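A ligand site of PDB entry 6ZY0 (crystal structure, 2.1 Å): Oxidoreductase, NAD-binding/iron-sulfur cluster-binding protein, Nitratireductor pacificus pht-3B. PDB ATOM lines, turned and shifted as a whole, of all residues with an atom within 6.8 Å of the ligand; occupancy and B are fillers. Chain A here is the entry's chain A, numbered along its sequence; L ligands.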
ATOM      1  N   SER A 499      15.178  17.121  -5.208  1.00  0.00           N
ATOM      2  CA  SER A 499      14.641  15.885  -5.751  1.00  0.00           C
ATOM      3  C   SER A 499      15.568  15.345  -6.830  1.00  0.00           C
ATOM      4  O   SER A 499      16.495  16.028  -7.285  1.00  0.00           O
ATOM      5  CB  SER A 499      13.233  16.106  -6.309  1.00  0.00           C
ATOM      6  OG  SER A 499      13.306  16.664  -7.610  1.00  0.00           O
ATOM      7  N   ARG A 500      15.306  14.108  -7.253  1.00  0.00           N
ATOM      8  CA  ARG A 500      16.144  13.492  -8.271  1.00  0.00           C
ATOM      9  C   ARG A 500      15.993  14.179  -9.622  1.00  0.00           C
ATOM     10  O   ARG A 500      16.956  14.212 -10.403  1.00  0.00           O
ATOM     11  CB  ARG A 500      15.833  12.003  -8.405  1.00  0.00           C
ATOM     12  CG  ARG A 500      16.612  11.299  -9.493  1.00  0.00           C
ATOM     13  CD  ARG A 500      16.262   9.832  -9.575  1.00  0.00           C
ATOM     14  NE  ARG A 500      16.613   9.123  -8.352  1.00  0.00           N
ATOM     15  CZ  ARG A 500      17.840   8.763  -8.022  1.00  0.00           C
ATOM     16  NH1 ARG A 500      18.865   9.056  -8.824  1.00  0.00           N
ATOM     17  NH2 ARG A 500      18.061   8.119  -6.880  1.00  0.00           N
ATOM     18  N   ILE A 501      14.815  14.744  -9.905  1.00  0.00           N
ATOM     19  CA  ILE A 501      14.605  15.413 -11.195  1.00  0.00           C
ATOM     20  C   ILE A 501      15.735  16.388 -11.482  1.00  0.00           C
ATOM     21  O   ILE A 501      16.120  16.583 -12.638  1.00  0.00           O
ATOM     22  CB  ILE A 501      13.225  16.119 -11.202  1.00  0.00           C
ATOM     23  CG1 ILE A 501      12.113  15.077 -11.079  1.00  0.00           C
ATOM     24  CG2 ILE A 501      13.030  16.908 -12.490  1.00  0.00           C
ATOM     25  CD1 ILE A 501      10.747  15.676 -10.932  1.00  0.00           C
ATOM     26  N   GLY A 502      16.308  16.984 -10.448  1.00  0.00           N
ATOM     27  CA  GLY A 502      17.564  17.678 -10.622  1.00  0.00           C
ATOM     28  C   GLY A 502      17.494  19.174 -10.431  1.00  0.00           C
ATOM     29  O   GLY A 502      17.895  19.711  -9.391  1.00  0.00           O
ATOM     30  N   THR A 504      14.672  20.700 -10.370  1.00  0.00           N
ATOM     31  CA  THR A 504      13.332  20.892  -9.859  1.00  0.00           C
ATOM     32  C   THR A 504      13.306  20.453  -8.401  1.00  0.00           C
ATOM     33  O   THR A 504      13.835  19.397  -8.041  1.00  0.00           O
ATOM     34  CB  THR A 504      12.290  20.081 -10.653  1.00  0.00           C
ATOM     35  OG1 THR A 504      12.345  20.470 -12.037  1.00  0.00           O
ATOM     36  CG2 THR A 504      10.909  20.355 -10.130  1.00  0.00           C
ATOM     37  N   LEU A 506      10.879  19.477  -5.034  1.00  0.00           N
ATOM     38  CA  LEU A 506       9.667  18.686  -4.901  1.00  0.00           C
ATOM     39  C   LEU A 506       8.971  19.082  -3.614  1.00  0.00           C
ATOM     40  O   LEU A 506       9.591  19.132  -2.549  1.00  0.00           O
ATOM     41  CB  LEU A 506       9.998  17.197  -4.907  1.00  0.00           C
ATOM     42  CG  LEU A 506       8.873  16.223  -5.192  1.00  0.00           C
ATOM     43  CD1 LEU A 506       9.432  15.089  -6.020  1.00  0.00           C
ATOM     44  CD2 LEU A 506       8.262  15.686  -3.908  1.00  0.00           C
ATOM     45  N   PRO A 512       6.308  17.468  -7.741  1.00  0.00           N
ATOM     46  CA  PRO A 512       7.125  18.342  -8.597  1.00  0.00           C
ATOM     47  C   PRO A 512       6.329  19.243  -9.522  1.00  0.00           C
ATOM     48  O   PRO A 512       6.918  19.825 -10.434  1.00  0.00           O
ATOM     49  CB  PRO A 512       7.920  17.318  -9.426  1.00  0.00           C
ATOM     50  CG  PRO A 512       6.983  16.182  -9.576  1.00  0.00           C
ATOM     51  CD  PRO A 512       6.093  16.147  -8.354  1.00  0.00           C
ATOM     52  N   LEU A 535      12.083  13.304   1.860  1.00  0.00           N
ATOM     53  CA  LEU A 535      12.204  13.092   0.421  1.00  0.00           C
ATOM     54  C   LEU A 535      13.573  12.558   0.026  1.00  0.00           C
ATOM     55  O   LEU A 535      13.686  11.838  -0.979  1.00  0.00           O
ATOM     56  CB  LEU A 535      11.949  14.399  -0.329  1.00  0.00           C
ATOM     57  CG  LEU A 535      11.988  14.199  -1.844  1.00  0.00           C
ATOM     58  CD1 LEU A 535      10.781  13.409  -2.283  1.00  0.00           C
ATOM     59  CD2 LEU A 535      12.090  15.513  -2.574  1.00  0.00           C
ATOM     60  N   PHE A 538      13.381   8.985   0.204  1.00  0.00           N
ATOM     61  CA  PHE A 538      12.419   8.530  -0.797  1.00  0.00           C
ATOM     62  C   PHE A 538      13.055   8.488  -2.184  1.00  0.00           C
ATOM     63  O   PHE A 538      12.921   7.488  -2.904  1.00  0.00           O
ATOM     64  CB  PHE A 538      11.197   9.428  -0.792  1.00  0.00           C
ATOM     65  CG  PHE A 538      10.024   8.854  -1.516  1.00  0.00           C
ATOM     66  CD1 PHE A 538       9.955   8.882  -2.901  1.00  0.00           C
ATOM     67  CD2 PHE A 538       8.977   8.283  -0.824  1.00  0.00           C
ATOM     68  CE1 PHE A 538       8.866   8.360  -3.567  1.00  0.00           C
ATOM     69  CE2 PHE A 538       7.891   7.750  -1.483  1.00  0.00           C
ATOM     70  CZ  PHE A 538       7.839   7.800  -2.864  1.00  0.00           C
ATOM     71  N   CYS A 539      13.758   9.548  -2.576  1.00  0.00           N
ATOM     72  CA  CYS A 539      14.339   9.574  -3.910  1.00  0.00           C
ATOM     73  C   CYS A 539      15.476   8.575  -4.055  1.00  0.00           C
ATOM     74  O   CYS A 539      15.738   8.101  -5.169  1.00  0.00           O
ATOM     75  CB  CYS A 539      14.822  10.985  -4.248  1.00  0.00           C
ATOM     76  SG  CYS A 539      13.537  12.064  -4.909  1.00  0.00           S
ATOM     77  N   ASN A 540      16.174   8.235  -2.961  1.00  0.00           N
ATOM     78  CA  ASN A 540      17.208   7.207  -3.059  1.00  0.00           C
ATOM     79  C   ASN A 540      16.636   5.861  -3.477  1.00  0.00           C
ATOM     80  O   ASN A 540      17.384   5.011  -3.961  1.00  0.00           O
ATOM     81  CB  ASN A 540      17.964   7.044  -1.740  1.00  0.00           C
ATOM     82  CG  ASN A 540      18.780   8.270  -1.375  1.00  0.00           C
ATOM     83  OD1 ASN A 540      19.965   8.350  -1.705  1.00  0.00           O
ATOM     84  ND2 ASN A 540      18.163   9.210  -0.673  1.00  0.00           N
ATOM     85  N   GLN A 541      15.327   5.660  -3.309  1.00  0.00           N
ATOM     86  CA  GLN A 541      14.678   4.397  -3.613  1.00  0.00           C
ATOM     87  C   GLN A 541      13.817   4.450  -4.868  1.00  0.00           C
ATOM     88  O   GLN A 541      13.099   3.495  -5.161  1.00  0.00           O
ATOM     89  CB  GLN A 541      13.814   3.959  -2.435  1.00  0.00           C
ATOM     90  CG  GLN A 541      14.497   3.999  -1.110  1.00  0.00           C
ATOM     91  CD  GLN A 541      13.613   3.507  -0.003  1.00  0.00           C
ATOM     92  OE1 GLN A 541      13.123   2.377  -0.040  1.00  0.00           O
ATOM     93  NE2 GLN A 541      13.399   4.357   0.994  1.00  0.00           N
ATOM     94  N   CYS A 542      13.863   5.557  -5.603  1.00  0.00           N
ATOM     95  CA  CYS A 542      12.972   5.789  -6.725  1.00  0.00           C
ATOM     96  C   CYS A 542      13.806   6.166  -7.939  1.00  0.00           C
ATOM     97  O   CYS A 542      14.823   6.856  -7.813  1.00  0.00           O
ATOM     98  CB  CYS A 542      11.957   6.895  -6.384  1.00  0.00           C
ATOM     99  SG  CYS A 542      10.551   7.048  -7.503  1.00  0.00           S
ATOM    100  N   ARG A 543      13.399   5.683  -9.113  1.00  0.00           N
ATOM    101  CA  ARG A 543      14.045   6.055 -10.364  1.00  0.00           C
ATOM    102  C   ARG A 543      13.036   6.420 -11.440  1.00  0.00           C
ATOM    103  O   ARG A 543      13.415   6.489 -12.611  1.00  0.00           O
ATOM    104  CB  ARG A 543      14.932   4.920 -10.876  1.00  0.00           C
ATOM    105  CG  ARG A 543      16.010   4.478  -9.915  1.00  0.00           C
ATOM    106  CD  ARG A 543      17.107   5.524  -9.781  1.00  0.00           C
ATOM    107  NE  ARG A 543      18.192   5.059  -8.920  1.00  0.00           N
ATOM    108  CZ  ARG A 543      18.124   5.026  -7.592  1.00  0.00           C
ATOM    109  NH1 ARG A 543      17.026   5.438  -6.968  1.00  0.00           N
ATOM    110  NH2 ARG A 543      19.163   4.592  -6.887  1.00  0.00           N
ATOM    111  N   LYS A 544      11.774   6.659 -11.079  1.00  0.00           N
ATOM    112  CA  LYS A 544      10.710   6.733 -12.078  1.00  0.00           C
ATOM    113  C   LYS A 544      10.950   7.876 -13.053  1.00  0.00           C
ATOM    114  O   LYS A 544      10.936   7.669 -14.276  1.00  0.00           O
ATOM    115  CB  LYS A 544       9.357   6.887 -11.384  1.00  0.00           C
ATOM    116  CG  LYS A 544       8.182   6.822 -12.335  1.00  0.00           C
ATOM    117  CD  LYS A 544       6.955   6.241 -11.678  1.00  0.00           C
ATOM    118  CE  LYS A 544       5.804   6.166 -12.683  1.00  0.00           C
ATOM    119  NZ  LYS A 544       4.657   5.371 -12.168  1.00  0.00           N
ATOM    120  N   CYS A 545      11.202   9.081 -12.541  1.00  0.00           N
ATOM    121  CA  CYS A 545      11.444  10.225 -13.415  1.00  0.00           C
ATOM    122  C   CYS A 545      12.647   9.975 -14.316  1.00  0.00           C
ATOM    123  O   CYS A 545      12.608  10.270 -15.511  1.00  0.00           O
ATOM    124  CB  CYS A 545      11.661  11.483 -12.583  1.00  0.00           C
ATOM    125  SG  CYS A 545      12.970  11.338 -11.342  1.00  0.00           S
ATOM    126  N   ALA A 546      13.729   9.426 -13.753  1.00  0.00           N
ATOM    127  CA  ALA A 546      14.900   9.115 -14.561  1.00  0.00           C
ATOM    128  C   ALA A 546      14.553   8.111 -15.652  1.00  0.00           C
ATOM    129  O   ALA A 546      15.013   8.239 -16.792  1.00  0.00           O
ATOM    130  CB  ALA A 546      16.018   8.566 -13.670  1.00  0.00           C
ATOM    131  N   ILE A 554      18.050  12.746 -16.536  1.00  0.00           N
ATOM    132  CA  ILE A 554      17.979  12.695 -15.081  1.00  0.00           C
ATOM    133  C   ILE A 554      18.920  11.604 -14.580  1.00  0.00           C
ATOM    134  O   ILE A 554      19.040  10.540 -15.193  1.00  0.00           O
ATOM    135  CB  ILE A 554      16.525  12.448 -14.623  1.00  0.00           C
ATOM    136  CG1 ILE A 554      15.662  13.676 -14.904  1.00  0.00           C
ATOM    137  CG2 ILE A 554      16.483  12.141 -13.147  1.00  0.00           C
ATOM    138  CD1 ILE A 554      14.184  13.460 -14.684  1.00  0.00           C
ATOM    139  N   TRP A 568      21.171  16.297  -6.973  1.00  0.00           N
ATOM    140  CA  TRP A 568      21.165  15.355  -8.087  1.00  0.00           C
ATOM    141  C   TRP A 568      21.312  16.181  -9.356  1.00  0.00           C
ATOM    142  O   TRP A 568      20.430  16.978  -9.683  1.00  0.00           O
ATOM    143  CB  TRP A 568      19.894  14.523  -8.144  1.00  0.00           C
ATOM    144  CG  TRP A 568      19.868  13.315  -7.261  1.00  0.00           C
ATOM    145  CD1 TRP A 568      20.502  12.120  -7.507  1.00  0.00           C
ATOM    146  CD2 TRP A 568      19.109  13.133  -6.068  1.00  0.00           C
ATOM    147  NE1 TRP A 568      20.219  11.225  -6.505  1.00  0.00           N
ATOM    148  CE2 TRP A 568      19.363  11.813  -5.613  1.00  0.00           C
ATOM    149  CE3 TRP A 568      18.255  13.949  -5.330  1.00  0.00           C
ATOM    150  CZ2 TRP A 568      18.792  11.310  -4.443  1.00  0.00           C
ATOM    151  CZ3 TRP A 568      17.694  13.441  -4.173  1.00  0.00           C
ATOM    152  CH2 TRP A 568      17.964  12.139  -3.736  1.00  0.00           C
ATOM    153  N   CYS A 591       8.913  14.652 -16.679  1.00  0.00           N
ATOM    154  CA  CYS A 591       9.457  14.275 -15.374  1.00  0.00           C
ATOM    155  C   CYS A 591       8.577  14.758 -14.212  1.00  0.00           C
ATOM    156  O   CYS A 591       8.507  14.081 -13.174  1.00  0.00           O
ATOM    157  CB  CYS A 591      10.895  14.784 -15.293  1.00  0.00           C
ATOM    158  SG  CYS A 591      11.078  16.583 -15.607  1.00  0.00           S
ATOM    159  N   MET A 594       5.580  12.082 -14.115  1.00  0.00           N
ATOM    160  CA  MET A 594       5.862  10.694 -13.802  1.00  0.00           C
ATOM    161  C   MET A 594       6.140  10.442 -12.325  1.00  0.00           C
ATOM    162  O   MET A 594       6.081   9.288 -11.895  1.00  0.00           O
ATOM    163  CB  MET A 594       7.038  10.204 -14.633  1.00  0.00           C
ATOM    164  CG  MET A 594       6.707  10.122 -16.106  1.00  0.00           C
ATOM    165  SD  MET A 594       5.315   9.011 -16.410  1.00  0.00           S
ATOM    166  CE  MET A 594       4.255  10.140 -17.257  1.00  0.00           C
ATOM    167  N   CYS A 595       6.421  11.476 -11.558  1.00  0.00           N
ATOM    168  CA  CYS A 595       6.797  11.272 -10.163  1.00  0.00           C
ATOM    169  C   CYS A 595       5.630  10.728  -9.352  1.00  0.00           C
ATOM    170  O   CYS A 595       4.480  11.161  -9.545  1.00  0.00           O
ATOM    171  CB  CYS A 595       7.279  12.594  -9.567  1.00  0.00           C
ATOM    172  SG  CYS A 595       7.714  12.487  -7.843  1.00  0.00           S
ATOM    173  N   PRO A 596       5.879   9.789  -8.428  1.00  0.00           N
ATOM    174  CA  PRO A 596       4.783   9.275  -7.590  1.00  0.00           C
ATOM    175  C   PRO A 596       4.102  10.348  -6.763  1.00  0.00           C
ATOM    176  O   PRO A 596       2.918  10.205  -6.429  1.00  0.00           O
ATOM    177  CB  PRO A 596       5.486   8.228  -6.709  1.00  0.00           C
ATOM    178  CG  PRO A 596       6.654   7.800  -7.502  1.00  0.00           C
ATOM    179  CD  PRO A 596       7.127   9.040  -8.214  1.00  0.00           C
ATOM    180  N   TRP A 597       4.823  11.416  -6.407  1.00  0.00           N
ATOM    181  CA  TRP A 597       4.238  12.520  -5.663  1.00  0.00           C
ATOM    182  C   TRP A 597       3.273  13.346  -6.495  1.00  0.00           C
ATOM    183  O   TRP A 597       2.544  14.180  -5.945  1.00  0.00           O
ATOM    184  CB  TRP A 597       5.356  13.423  -5.125  1.00  0.00           C
ATOM    185  CG  TRP A 597       6.258  12.736  -4.145  1.00  0.00           C
ATOM    186  CD1 TRP A 597       7.344  11.965  -4.423  1.00  0.00           C
ATOM    187  CD2 TRP A 597       6.156  12.791  -2.711  1.00  0.00           C
ATOM    188  NE1 TRP A 597       7.916  11.520  -3.260  1.00  0.00           N
ATOM    189  CE2 TRP A 597       7.204  12.009  -2.193  1.00  0.00           C
ATOM    190  CE3 TRP A 597       5.277  13.415  -1.821  1.00  0.00           C
ATOM    191  CZ2 TRP A 597       7.405  11.839  -0.816  1.00  0.00           C
ATOM    192  CZ3 TRP A 597       5.475  13.240  -0.452  1.00  0.00           C
ATOM    193  CH2 TRP A 597       6.529  12.460   0.024  1.00  0.00           C
ATOM    194  N   ASN A 598       3.261  13.160  -7.810  1.00  0.00           N
ATOM    195  CA  ASN A 598       2.254  13.796  -8.651  1.00  0.00           C
ATOM    196  C   ASN A 598       0.951  13.027  -8.459  1.00  0.00           C
ATOM    197  O   ASN A 598       0.734  11.984  -9.080  1.00  0.00           O
ATOM    198  CB  ASN A 598       2.687  13.792 -10.110  1.00  0.00           C
ATOM    199  CG  ASN A 598       1.708  14.489 -11.015  1.00  0.00           C
ATOM    200  OD1 ASN A 598       1.272  15.601 -10.728  1.00  0.00           O
ATOM    201  ND2 ASN A 598       1.348  13.844 -12.126  1.00  0.00           N
ATOM    202  N   ILE A 623       6.603   3.304  -3.873  1.00  0.00           N
ATOM    203  CA  ILE A 623       7.357   3.488  -5.116  1.00  0.00           C
ATOM    204  C   ILE A 623       7.035   2.368  -6.101  1.00  0.00           C
ATOM    205  O   ILE A 623       6.800   2.621  -7.292  1.00  0.00           O
ATOM    206  CB  ILE A 623       8.862   3.556  -4.816  1.00  0.00           C
ATOM    207  CG1 ILE A 623       9.206   4.876  -4.126  1.00  0.00           C
ATOM    208  CG2 ILE A 623       9.642   3.388  -6.086  1.00  0.00           C
ATOM    209  CD1 ILE A 623      10.542   4.880  -3.426  1.00  0.00           C
HETATM  210 FE1  LIG L   1      12.166  11.164  -9.276  1.00  0.00          FE
HETATM  211 FE2  LIG L   1      10.906   9.279  -7.770  1.00  0.00          FE
HETATM  212 FE3  LIG L   1       9.851  11.787  -7.998  1.00  0.00          FE
HETATM  213 FE4  LIG L   1      12.115  11.418  -6.564  1.00  0.00          FE
HETATM  214  S1  LIG L   1      10.057  10.578  -6.091  1.00  0.00           S
HETATM  215  S2  LIG L   1      11.733  13.055  -8.055  1.00  0.00           S
HETATM  216  S3  LIG L   1      13.118   9.761  -7.785  1.00  0.00           S
HETATM  217  S4  LIG L   1      10.128  10.253  -9.663  1.00  0.00           S
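Residues that only touch the ligand: Pro 596, Phe 538, Ile 501, Leu 506, Ser 499 and Lys 544.
Hydrophobic or aromatic side chains that line the ligand: Ile 501, Leu 506, Phe 538, Pro 596 and Trp 597.
Of the 26 residues printed, 12 come within 4 Å of the ligand.
The side-chain sulfur (SG) of Cys 595 sits close to the backbone NH (N) of Trp 597.
O of Cys 542 sits at hydrogen-bond distance from NE of Arg 500, at 2.9 Å.
The backbone NH of Lys 544 sits close to the side-chain sulfur of Cys 542 (3.8 Å).
The backbone carbonyl oxygen (O) of Cys 539 sits at hydrogen-bond distance from the guanidinium group (NH2) of Arg 500.
The backbone carbonyl oxygen (O) of Cys 539 is in hydrogen-bond range of the guanidinium group (NH1) of Arg 543 (3.5 Å).
N of Ile 501 sits close to OG of Ser 499 (3.4 Å).
The side-chain hydroxyl (OG) of Ser 499 lies within hydrogen-bond range of the backbone carbonyl oxygen (O) of Thr 504 (2.8 Å).
The backbone NH (N) of Cys 545 lies close to a sulfur (S4) of the ligand.
FE1 of the ligand is bound by SG of Cys 545.
FE3 of the ligand is bound by SG of Cys 595 (2.3 Å).
FE2 of the ligand is bound by SG of Cys 542.
FE4 of the ligand is bound by SG of Cys 539 (2.3 Å).
The indole nitrogen (NE1) of Trp 597 sits close to a sulfur (S1) of the ligand, 3.7 Å away.
NE of Arg 500 sits close to S3 of the ligand.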
